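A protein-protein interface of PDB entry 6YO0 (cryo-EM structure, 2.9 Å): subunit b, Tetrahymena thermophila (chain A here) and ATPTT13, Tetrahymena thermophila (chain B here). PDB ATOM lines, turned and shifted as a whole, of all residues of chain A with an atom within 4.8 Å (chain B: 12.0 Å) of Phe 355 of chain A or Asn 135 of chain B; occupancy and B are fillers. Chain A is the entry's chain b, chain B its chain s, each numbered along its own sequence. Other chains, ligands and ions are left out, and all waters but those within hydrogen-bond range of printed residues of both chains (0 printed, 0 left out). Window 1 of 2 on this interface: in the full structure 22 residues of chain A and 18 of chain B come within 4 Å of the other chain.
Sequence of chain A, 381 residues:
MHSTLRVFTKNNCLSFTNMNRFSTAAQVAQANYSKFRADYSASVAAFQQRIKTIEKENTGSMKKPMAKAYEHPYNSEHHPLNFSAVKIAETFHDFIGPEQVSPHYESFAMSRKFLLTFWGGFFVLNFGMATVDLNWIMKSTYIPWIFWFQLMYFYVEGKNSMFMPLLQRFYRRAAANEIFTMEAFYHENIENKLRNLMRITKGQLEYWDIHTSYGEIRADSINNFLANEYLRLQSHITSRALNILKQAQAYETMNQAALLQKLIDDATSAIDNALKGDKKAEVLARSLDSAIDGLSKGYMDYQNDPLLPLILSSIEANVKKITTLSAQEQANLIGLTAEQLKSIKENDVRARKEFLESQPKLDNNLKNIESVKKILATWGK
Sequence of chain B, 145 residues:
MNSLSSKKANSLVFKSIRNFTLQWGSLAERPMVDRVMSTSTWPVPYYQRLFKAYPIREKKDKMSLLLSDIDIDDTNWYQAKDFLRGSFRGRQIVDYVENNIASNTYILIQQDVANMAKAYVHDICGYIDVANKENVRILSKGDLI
Hydrophobic or aromatic side chains of chain A that line the printed part of chain B: Leu 233, Phe 355 and Leu 356. Of the 18 printed residues of chain B, 7 touch a printed residue of chain A. Hydrophobic or aromatic side chains of chain B within 4 Å of the printed part of chain A: Ala 131, Val 136 and Leu 139. Along chain B the printed residues that touch a printed residue of chain A span positions 131 to 143. Among the printed residues, 10 pairs touch across the chains. Among the printed residues, no Asp or Glu carboxylate lies within 4 Å of a Lys or Arg side-chain nitrogen of the other chain.
The side-chain amide nitrogen of Asn 132 of chain B sits at hydrogen-bond distance from the side-chain carboxylate of Asp 129 of chain B. The side-chain amide nitrogen (ND2) of Asn 135 of chain B sits close to the backbone carbonyl oxygen (O) of Ala 131 of chain B. The backbone carbonyl oxygen of Val 136 of chain B sits at hydrogen-bond distance from the side-chain hydroxyl of Ser 140 of chain B, 2.6 Å away. The side-chain carboxylate of Glu 229 of chain A lies within salt-bridge range of the guanidinium group of Arg 232 of chain A, at 2.5 Å. The backbone carbonyl oxygen (O) of Phe 355 of chain A lies within hydrogen-bond range of the side-chain hydroxyl (OG) of Ser 358 of chain A.
Among the printed residues, pairs that only touch across the chains: Leu 233 of chain A with Asn 135 of chain B, Leu 356 of chain A with Val 136 of chain B, Arg 352 of chain A with Asp 143 of chain B, Leu 356 of chain A with Leu 139 of chain B, Glu 229 of chain A with Ala 131 of chain B, Phe 355 of chain A with Leu 139 of chain B and Phe 355 of chain A with Asn 135 of chain B.
No residue of chain B comes within 4 Å of Ala 351 of chain A. Of the printed residues of chain B, Arg 352 of chain A touches Leu 139 (2.7 Å), Gly 142 (2.7 Å) and Asp 143 (3.4 Å). Of chain B, only Asn 132, Val 136 and Leu 139 come within 4 Å of Leu 356 of chain A. Glu 357 of chain A touches none of the printed residues of chain B. No residue of chain B comes within 4 Å of Ser 358 of chain A. Printed residues of chain A within 4 Å of Asn 132 of chain B: Leu 356 (3.5 Å). Asn 135 of chain B touches just these residues of chain A: Leu 233 and Phe 355. Printed residues of chain A within 4 Å of Leu 139 of chain B: Arg 352 (2.7 Å), Phe 355 (3.7 Å) and Leu 356 (3.5 Å). Lys 141 of chain B touches none of the printed residues of chain A. The nearest printed residue of chain B that does not touch Arg 352 of chain A is Ser 140 of chain B (4.4 Å).
OD1 of Asn 132 of chain B lies close to O of Leu 356 of chain A (3.5 Å). NH2 of Arg 352 of chain A sits at hydrogen-bond distance from O of Leu 139 of chain B (2.7 Å). The backbone carbonyl oxygen (O) of Gly 142 of chain B is in hydrogen-bond range of the guanidinium group (NH2) of Arg 352 of chain A (2.7 Å).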
ATOM      1  N   GLU A 229       2.914  19.029  16.439  1.00  0.00           N
ATOM      2  CA  GLU A 229       4.225  18.961  15.805  1.00  0.00           C
ATOM      3  C   GLU A 229       4.605  20.304  15.198  1.00  0.00           C
ATOM      4  O   GLU A 229       5.772  20.707  15.243  1.00  0.00           O
ATOM      5  CB  GLU A 229       4.229  17.869  14.740  1.00  0.00           C
ATOM      6  CG  GLU A 229       5.609  17.461  14.279  1.00  0.00           C
ATOM      7  CD  GLU A 229       6.375  16.689  15.333  1.00  0.00           C
ATOM      8  OE1 GLU A 229       5.919  16.643  16.495  1.00  0.00           O
ATOM      9  OE2 GLU A 229       7.437  16.124  14.998  1.00  0.00           O
ATOM     10  N   ARG A 232       5.840  22.389  17.979  1.00  0.00           N
ATOM     11  CA  ARG A 232       7.184  22.002  18.394  1.00  0.00           C
ATOM     12  C   ARG A 232       8.227  22.535  17.426  1.00  0.00           C
ATOM     13  O   ARG A 232       9.304  22.979  17.839  1.00  0.00           O
ATOM     14  CB  ARG A 232       7.294  20.482  18.480  1.00  0.00           C
ATOM     15  CG  ARG A 232       8.617  20.005  19.045  1.00  0.00           C
ATOM     16  CD  ARG A 232       8.621  18.506  19.292  1.00  0.00           C
ATOM     17  NE  ARG A 232       8.578  17.749  18.043  1.00  0.00           N
ATOM     18  CZ  ARG A 232       9.654  17.283  17.411  1.00  0.00           C
ATOM     19  NH1 ARG A 232      10.869  17.494  17.898  1.00  0.00           N
ATOM     20  NH2 ARG A 232       9.517  16.604  16.282  1.00  0.00           N
ATOM     21  N   LEU A 233       7.922  22.502  16.130  1.00  0.00           N
ATOM     22  CA  LEU A 233       8.855  23.022  15.141  1.00  0.00           C
ATOM     23  C   LEU A 233       9.020  24.528  15.277  1.00  0.00           C
ATOM     24  O   LEU A 233      10.133  25.051  15.149  1.00  0.00           O
ATOM     25  CB  LEU A 233       8.369  22.661  13.741  1.00  0.00           C
ATOM     26  CG  LEU A 233       9.157  23.242  12.567  1.00  0.00           C
ATOM     27  CD1 LEU A 233       9.079  22.299  11.387  1.00  0.00           C
ATOM     28  CD2 LEU A 233       8.643  24.620  12.181  1.00  0.00           C
ATOM     29  N   HIS A 236      11.344  25.131  18.017  1.00  0.00           N
ATOM     30  CA  HIS A 236      12.698  24.783  17.607  1.00  0.00           C
ATOM     31  C   HIS A 236      13.331  25.878  16.762  1.00  0.00           C
ATOM     32  O   HIS A 236      14.515  26.193  16.927  1.00  0.00           O
ATOM     33  CB  HIS A 236      12.672  23.466  16.840  1.00  0.00           C
ATOM     34  CG  HIS A 236      13.980  23.106  16.215  1.00  0.00           C
ATOM     35  ND1 HIS A 236      14.319  23.493  14.939  1.00  0.00           N
ATOM     36  CD2 HIS A 236      15.036  22.405  16.691  1.00  0.00           C
ATOM     37  CE1 HIS A 236      15.524  23.037  14.650  1.00  0.00           C
ATOM     38  NE2 HIS A 236      15.983  22.376  15.696  1.00  0.00           N
ATOM     39  N   ALA A 351      22.252  21.569  14.894  1.00  0.00           N
ATOM     40  CA  ALA A 351      20.916  21.616  15.472  1.00  0.00           C
ATOM     41  C   ALA A 351      19.893  21.067  14.492  1.00  0.00           C
ATOM     42  O   ALA A 351      19.009  20.289  14.873  1.00  0.00           O
ATOM     43  CB  ALA A 351      20.566  23.047  15.866  1.00  0.00           C
ATOM     44  N   ARG A 352      19.992  21.465  13.225  1.00  0.00           N
ATOM     45  CA  ARG A 352      19.079  20.940  12.218  1.00  0.00           C
ATOM     46  C   ARG A 352      19.192  19.424  12.137  1.00  0.00           C
ATOM     47  O   ARG A 352      18.183  18.713  12.171  1.00  0.00           O
ATOM     48  CB  ARG A 352      19.386  21.581  10.864  1.00  0.00           C
ATOM     49  CG  ARG A 352      18.724  20.916   9.674  1.00  0.00           C
ATOM     50  CD  ARG A 352      19.209  21.535   8.377  1.00  0.00           C
ATOM     51  NE  ARG A 352      18.747  22.911   8.224  1.00  0.00           N
ATOM     52  CZ  ARG A 352      19.001  23.671   7.165  1.00  0.00           C
ATOM     53  NH1 ARG A 352      19.720  23.194   6.158  1.00  0.00           N
ATOM     54  NH2 ARG A 352      18.537  24.911   7.110  1.00  0.00           N
ATOM     55  N   LYS A 353      20.419  18.906  12.058  1.00  0.00           N
ATOM     56  CA  LYS A 353      20.583  17.461  11.953  1.00  0.00           C
ATOM     57  C   LYS A 353      20.049  16.770  13.196  1.00  0.00           C
ATOM     58  O   LYS A 353      19.420  15.711  13.107  1.00  0.00           O
ATOM     59  CB  LYS A 353      22.054  17.103  11.749  1.00  0.00           C
ATOM     60  CG  LYS A 353      22.765  17.759  10.565  1.00  0.00           C
ATOM     61  CD  LYS A 353      22.171  17.414   9.202  1.00  0.00           C
ATOM     62  CE  LYS A 353      20.985  18.291   8.824  1.00  0.00           C
ATOM     63  NZ  LYS A 353      20.492  17.986   7.451  1.00  0.00           N
ATOM     64  N   GLU A 354      20.258  17.370  14.365  1.00  0.00           N
ATOM     65  CA  GLU A 354      19.771  16.743  15.584  1.00  0.00           C
ATOM     66  C   GLU A 354      18.250  16.749  15.625  1.00  0.00           C
ATOM     67  O   GLU A 354      17.631  15.760  16.031  1.00  0.00           O
ATOM     68  CB  GLU A 354      20.352  17.459  16.801  1.00  0.00           C
ATOM     69  CG  GLU A 354      20.048  16.789  18.130  1.00  0.00           C
ATOM     70  CD  GLU A 354      18.661  17.114  18.654  1.00  0.00           C
ATOM     71  OE1 GLU A 354      18.061  18.106  18.188  1.00  0.00           O
ATOM     72  OE2 GLU A 354      18.170  16.376  19.534  1.00  0.00           O
ATOM     73  N   PHE A 355      17.629  17.852  15.204  1.00  0.00           N
ATOM     74  CA  PHE A 355      16.173  17.909  15.195  1.00  0.00           C
ATOM     75  C   PHE A 355      15.592  16.966  14.151  1.00  0.00           C
ATOM     76  O   PHE A 355      14.540  16.356  14.375  1.00  0.00           O
ATOM     77  CB  PHE A 355      15.709  19.342  14.949  1.00  0.00           C
ATOM     78  CG  PHE A 355      14.219  19.488  14.846  1.00  0.00           C
ATOM     79  CD1 PHE A 355      13.442  19.575  15.986  1.00  0.00           C
ATOM     80  CD2 PHE A 355      13.598  19.554  13.614  1.00  0.00           C
ATOM     81  CE1 PHE A 355      12.073  19.716  15.898  1.00  0.00           C
ATOM     82  CE2 PHE A 355      12.228  19.695  13.521  1.00  0.00           C
ATOM     83  CZ  PHE A 355      11.466  19.779  14.665  1.00  0.00           C
ATOM     84  N   LEU A 356      16.261  16.830  13.004  1.00  0.00           N
ATOM     85  CA  LEU A 356      15.742  15.965  11.952  1.00  0.00           C
ATOM     86  C   LEU A 356      16.048  14.501  12.238  1.00  0.00           C
ATOM     87  O   LEU A 356      15.137  13.668  12.280  1.00  0.00           O
ATOM     88  CB  LEU A 356      16.318  16.367  10.594  1.00  0.00           C
ATOM     89  CG  LEU A 356      15.620  17.502   9.838  1.00  0.00           C
ATOM     90  CD1 LEU A 356      14.163  17.158   9.574  1.00  0.00           C
ATOM     91  CD2 LEU A 356      15.734  18.821  10.564  1.00  0.00           C
ATOM     92  N   GLU A 357      17.324  14.168  12.450  1.00  0.00           N
ATOM     93  CA  GLU A 357      17.683  12.774  12.680  1.00  0.00           C
ATOM     94  C   GLU A 357      17.042  12.220  13.943  1.00  0.00           C
ATOM     95  O   GLU A 357      16.997  10.998  14.116  1.00  0.00           O
ATOM     96  CB  GLU A 357      19.205  12.612  12.737  1.00  0.00           C
ATOM     97  CG  GLU A 357      19.954  13.242  11.568  1.00  0.00           C
ATOM     98  CD  GLU A 357      19.464  12.750  10.221  1.00  0.00           C
ATOM     99  OE1 GLU A 357      18.847  11.667  10.168  1.00  0.00           O
ATOM    100  OE2 GLU A 357      19.696  13.451   9.213  1.00  0.00           O
ATOM    101  N   SER A 358      16.553  13.086  14.828  1.00  0.00           N
ATOM    102  CA  SER A 358      15.867  12.619  16.024  1.00  0.00           C
ATOM    103  C   SER A 358      14.720  11.712  15.614  1.00  0.00           C
ATOM    104  O   SER A 358      13.770  12.156  14.962  1.00  0.00           O
ATOM    105  CB  SER A 358      15.349  13.801  16.835  1.00  0.00           C
ATOM    106  OG  SER A 358      14.447  14.579  16.069  1.00  0.00           O
ATOM    107  N   TYR B 127       1.306   5.836   7.932  1.00  0.00           N
ATOM    108  CA  TYR B 127       1.175   7.279   7.790  1.00  0.00           C
ATOM    109  C   TYR B 127       2.062   8.046   8.762  1.00  0.00           C
ATOM    110  O   TYR B 127       1.833   9.240   8.990  1.00  0.00           O
ATOM    111  CB  TYR B 127      -0.286   7.693   7.980  1.00  0.00           C
ATOM    112  CG  TYR B 127      -1.200   7.350   6.819  1.00  0.00           C
ATOM    113  CD1 TYR B 127      -2.578   7.321   6.985  1.00  0.00           C
ATOM    114  CD2 TYR B 127      -0.689   7.052   5.558  1.00  0.00           C
ATOM    115  CE1 TYR B 127      -3.420   7.009   5.932  1.00  0.00           C
ATOM    116  CE2 TYR B 127      -1.523   6.742   4.502  1.00  0.00           C
ATOM    117  CZ  TYR B 127      -2.885   6.721   4.694  1.00  0.00           C
ATOM    118  OH  TYR B 127      -3.713   6.410   3.638  1.00  0.00           O
ATOM    119  N   ILE B 128       3.063   7.390   9.341  1.00  0.00           N
ATOM    120  CA  ILE B 128       4.074   8.062  10.145  1.00  0.00           C
ATOM    121  C   ILE B 128       5.065   8.701   9.180  1.00  0.00           C
ATOM    122  O   ILE B 128       5.038   8.417   7.978  1.00  0.00           O
ATOM    123  CB  ILE B 128       4.762   7.069  11.098  1.00  0.00           C
ATOM    124  CG1 ILE B 128       5.603   7.792  12.150  1.00  0.00           C
ATOM    125  CG2 ILE B 128       5.658   6.133  10.315  1.00  0.00           C
ATOM    126  CD1 ILE B 128       6.301   6.849  13.099  1.00  0.00           C
ATOM    127  N   ASP B 129       5.936   9.570   9.688  1.00  0.00           N
ATOM    128  CA  ASP B 129       7.010  10.223   8.945  1.00  0.00           C
ATOM    129  C   ASP B 129       6.505  11.398   8.120  1.00  0.00           C
ATOM    130  O   ASP B 129       7.319  12.082   7.489  1.00  0.00           O
ATOM    131  CB  ASP B 129       7.737   9.243   8.009  1.00  0.00           C
ATOM    132  CG  ASP B 129       9.027   9.806   7.445  1.00  0.00           C
ATOM    133  OD1 ASP B 129       9.507  10.839   7.951  1.00  0.00           O
ATOM    134  OD2 ASP B 129       9.564   9.207   6.489  1.00  0.00           O
ATOM    135  N   VAL B 130       5.201  11.664   8.102  1.00  0.00           N
ATOM    136  CA  VAL B 130       4.689  12.775   7.305  1.00  0.00           C
ATOM    137  C   VAL B 130       5.246  14.097   7.820  1.00  0.00           C
ATOM    138  O   VAL B 130       5.860  14.868   7.074  1.00  0.00           O
ATOM    139  CB  VAL B 130       3.148  12.780   7.303  1.00  0.00           C
ATOM    140  CG1 VAL B 130       2.579  12.737   8.722  1.00  0.00           C
ATOM    141  CG2 VAL B 130       2.629  14.002   6.573  1.00  0.00           C
ATOM    142  N   ALA B 131       5.042  14.376   9.108  1.00  0.00           N
ATOM    143  CA  ALA B 131       5.550  15.615   9.682  1.00  0.00           C
ATOM    144  C   ALA B 131       7.066  15.705   9.603  1.00  0.00           C
ATOM    145  O   ALA B 131       7.612  16.799   9.419  1.00  0.00           O
ATOM    146  CB  ALA B 131       5.091  15.746  11.130  1.00  0.00           C
ATOM    147  N   ASN B 132       7.768  14.577   9.732  1.00  0.00           N
ATOM    148  CA  ASN B 132       9.222  14.614   9.630  1.00  0.00           C
ATOM    149  C   ASN B 132       9.660  15.035   8.235  1.00  0.00           C
ATOM    150  O   ASN B 132      10.576  15.852   8.084  1.00  0.00           O
ATOM    151  CB  ASN B 132       9.806  13.251   9.990  1.00  0.00           C
ATOM    152  CG  ASN B 132      11.305  13.189   9.792  1.00  0.00           C
ATOM    153  OD1 ASN B 132      12.071  13.695  10.611  1.00  0.00           O
ATOM    154  ND2 ASN B 132      11.733  12.574   8.697  1.00  0.00           N
ATOM    155  N   LYS B 133       9.010  14.498   7.202  1.00  0.00           N
ATOM    156  CA  LYS B 133       9.341  14.898   5.840  1.00  0.00           C
ATOM    157  C   LYS B 133       8.979  16.356   5.602  1.00  0.00           C
ATOM    158  O   LYS B 133       9.718  17.088   4.932  1.00  0.00           O
ATOM    159  CB  LYS B 133       8.626  13.996   4.838  1.00  0.00           C
ATOM    160  CG  LYS B 133       8.914  14.349   3.395  1.00  0.00           C
ATOM    161  CD  LYS B 133       8.222  13.398   2.441  1.00  0.00           C
ATOM    162  CE  LYS B 133       8.525  13.756   0.997  1.00  0.00           C
ATOM    163  NZ  LYS B 133       8.083  15.136   0.656  1.00  0.00           N
ATOM    164  N   GLU B 134       7.844  16.794   6.148  1.00  0.00           N
ATOM    165  CA  GLU B 134       7.459  18.197   6.053  1.00  0.00           C
ATOM    166  C   GLU B 134       8.540  19.091   6.640  1.00  0.00           C
ATOM    167  O   GLU B 134       8.934  20.093   6.033  1.00  0.00           O
ATOM    168  CB  GLU B 134       6.128  18.415   6.774  1.00  0.00           C
ATOM    169  CG  GLU B 134       5.628  19.848   6.764  1.00  0.00           C
ATOM    170  CD  GLU B 134       5.119  20.273   5.408  1.00  0.00           C
ATOM    171  OE1 GLU B 134       5.148  19.443   4.474  1.00  0.00           O
ATOM    172  OE2 GLU B 134       4.690  21.438   5.268  1.00  0.00           O
ATOM    173  N   ASN B 135       9.041  18.734   7.822  1.00  0.00           N
ATOM    174  CA  ASN B 135      10.092  19.529   8.444  1.00  0.00           C
ATOM    175  C   ASN B 135      11.346  19.541   7.582  1.00  0.00           C
ATOM    176  O   ASN B 135      12.011  20.576   7.456  1.00  0.00           O
ATOM    177  CB  ASN B 135      10.399  18.987   9.837  1.00  0.00           C
ATOM    178  CG  ASN B 135       9.160  18.879  10.703  1.00  0.00           C
ATOM    179  OD1 ASN B 135       8.185  19.604  10.503  1.00  0.00           O
ATOM    180  ND2 ASN B 135       9.191  17.976  11.675  1.00  0.00           N
ATOM    181  N   VAL B 136      11.683  18.404   6.973  1.00  0.00           N
ATOM    182  CA  VAL B 136      12.864  18.349   6.116  1.00  0.00           C
ATOM    183  C   VAL B 136      12.766  19.402   5.020  1.00  0.00           C
ATOM    184  O   VAL B 136      13.703  20.176   4.791  1.00  0.00           O
ATOM    185  CB  VAL B 136      13.035  16.940   5.521  1.00  0.00           C
ATOM    186  CG1 VAL B 136      14.138  16.939   4.483  1.00  0.00           C
ATOM    187  CG2 VAL B 136      13.345  15.938   6.611  1.00  0.00           C
ATOM    188  N   ARG B 137      11.629  19.445   4.327  1.00  0.00           N
ATOM    189  CA  ARG B 137      11.450  20.434   3.270  1.00  0.00           C
ATOM    190  C   ARG B 137      11.523  21.851   3.825  1.00  0.00           C
ATOM    191  O   ARG B 137      12.288  22.686   3.328  1.00  0.00           O
ATOM    192  CB  ARG B 137      10.117  20.203   2.561  1.00  0.00           C
ATOM    193  CG  ARG B 137       9.771  21.277   1.548  1.00  0.00           C
ATOM    194  CD  ARG B 137       8.479  20.966   0.818  1.00  0.00           C
ATOM    195  NE  ARG B 137       7.339  20.872   1.723  1.00  0.00           N
ATOM    196  CZ  ARG B 137       6.138  20.428   1.364  1.00  0.00           C
ATOM    197  NH1 ARG B 137       5.917  20.027   0.121  1.00  0.00           N
ATOM    198  NH2 ARG B 137       5.158  20.380   2.251  1.00  0.00           N
ATOM    199  N   ILE B 138      10.731  22.143   4.859  1.00  0.00           N
ATOM    200  CA  ILE B 138      10.672  23.506   5.377  1.00  0.00           C
ATOM    201  C   ILE B 138      12.034  23.944   5.893  1.00  0.00           C
ATOM    202  O   ILE B 138      12.435  25.102   5.725  1.00  0.00           O
ATOM    203  CB  ILE B 138       9.592  23.622   6.468  1.00  0.00           C
ATOM    204  CG1 ILE B 138       8.232  23.198   5.909  1.00  0.00           C
ATOM    205  CG2 ILE B 138       9.558  25.040   7.006  1.00  0.00           C
ATOM    206  CD1 ILE B 138       7.114  23.172   6.934  1.00  0.00           C
ATOM    207  N   LEU B 139      12.765  23.035   6.535  1.00  0.00           N
ATOM    208  CA  LEU B 139      14.045  23.408   7.122  1.00  0.00           C
ATOM    209  C   LEU B 139      15.160  23.363   6.089  1.00  0.00           C
ATOM    210  O   LEU B 139      16.121  24.135   6.185  1.00  0.00           O
ATOM    211  CB  LEU B 139      14.360  22.502   8.312  1.00  0.00           C
ATOM    212  CG  LEU B 139      13.312  22.514   9.431  1.00  0.00           C
ATOM    213  CD1 LEU B 139      13.781  21.723  10.636  1.00  0.00           C
ATOM    214  CD2 LEU B 139      12.978  23.938   9.838  1.00  0.00           C
ATOM    215  N   SER B 140      15.049  22.478   5.100  1.00  0.00           N
ATOM    216  CA  SER B 140      15.954  22.507   3.959  1.00  0.00           C
ATOM    217  C   SER B 140      15.684  23.694   3.047  1.00  0.00           C
ATOM    218  O   SER B 140      16.509  23.988   2.176  1.00  0.00           O
ATOM    219  CB  SER B 140      15.838  21.207   3.165  1.00  0.00           C
ATOM    220  OG  SER B 140      16.128  20.087   3.983  1.00  0.00           O
ATOM    221  N   LYS B 141      14.549  24.374   3.226  1.00  0.00           N
ATOM    222  CA  LYS B 141      14.246  25.570   2.449  1.00  0.00           C
ATOM    223  C   LYS B 141      15.367  26.593   2.567  1.00  0.00           C
ATOM    224  O   LYS B 141      15.997  26.974   1.575  1.00  0.00           O
ATOM    225  CB  LYS B 141      12.928  26.176   2.935  1.00  0.00           C
ATOM    226  CG  LYS B 141      12.555  27.504   2.290  1.00  0.00           C
ATOM    227  CD  LYS B 141      12.454  27.416   0.777  1.00  0.00           C
ATOM    228  CE  LYS B 141      11.533  26.292   0.337  1.00  0.00           C
ATOM    229  NZ  LYS B 141      10.187  26.414   0.962  1.00  0.00           N
ATOM    230  N   GLY B 142      15.626  27.045   3.791  1.00  0.00           N
ATOM    231  CA  GLY B 142      16.626  28.060   4.033  1.00  0.00           C
ATOM    232  C   GLY B 142      17.437  27.712   5.263  1.00  0.00           C
ATOM    233  O   GLY B 142      16.999  26.954   6.132  1.00  0.00           O
ATOM    234  N   ASP B 143      18.633  28.283   5.322  1.00  0.00           N
ATOM    235  CA  ASP B 143      19.520  28.113   6.463  1.00  0.00           C
ATOM    236  C   ASP B 143      19.478  29.406   7.264  1.00  0.00           C
ATOM    237  O   ASP B 143      19.789  30.482   6.741  1.00  0.00           O
ATOM    238  CB  ASP B 143      20.944  27.784   6.019  1.00  0.00           C
ATOM    239  CG  ASP B 143      21.880  27.556   7.185  1.00  0.00           C
ATOM    240  OD1 ASP B 143      21.422  27.643   8.345  1.00  0.00           O
ATOM    241  OD2 ASP B 143      23.076  27.289   6.947  1.00  0.00           O
ATOM    242  N   LEU B 144      19.088  29.287   8.533  1.00  0.00           N
ATOM    243  CA  LEU B 144      18.878  30.456   9.379  1.00  0.00           C
ATOM    244  C   LEU B 144      20.113  31.347   9.426  1.00  0.00           C
ATOM    245  O   LEU B 144      20.074  32.502   8.985  1.00  0.00           O
ATOM    246  CB  LEU B 144      18.487  29.994  10.780  1.00  0.00           C
ATOM    247  CG  LEU B 144      18.142  31.086  11.782  1.00  0.00           C
ATOM    248  CD1 LEU B 144      17.035  31.972  11.231  1.00  0.00           C
ATOM    249  CD2 LEU B 144      17.731  30.450  13.091  1.00  0.00           C
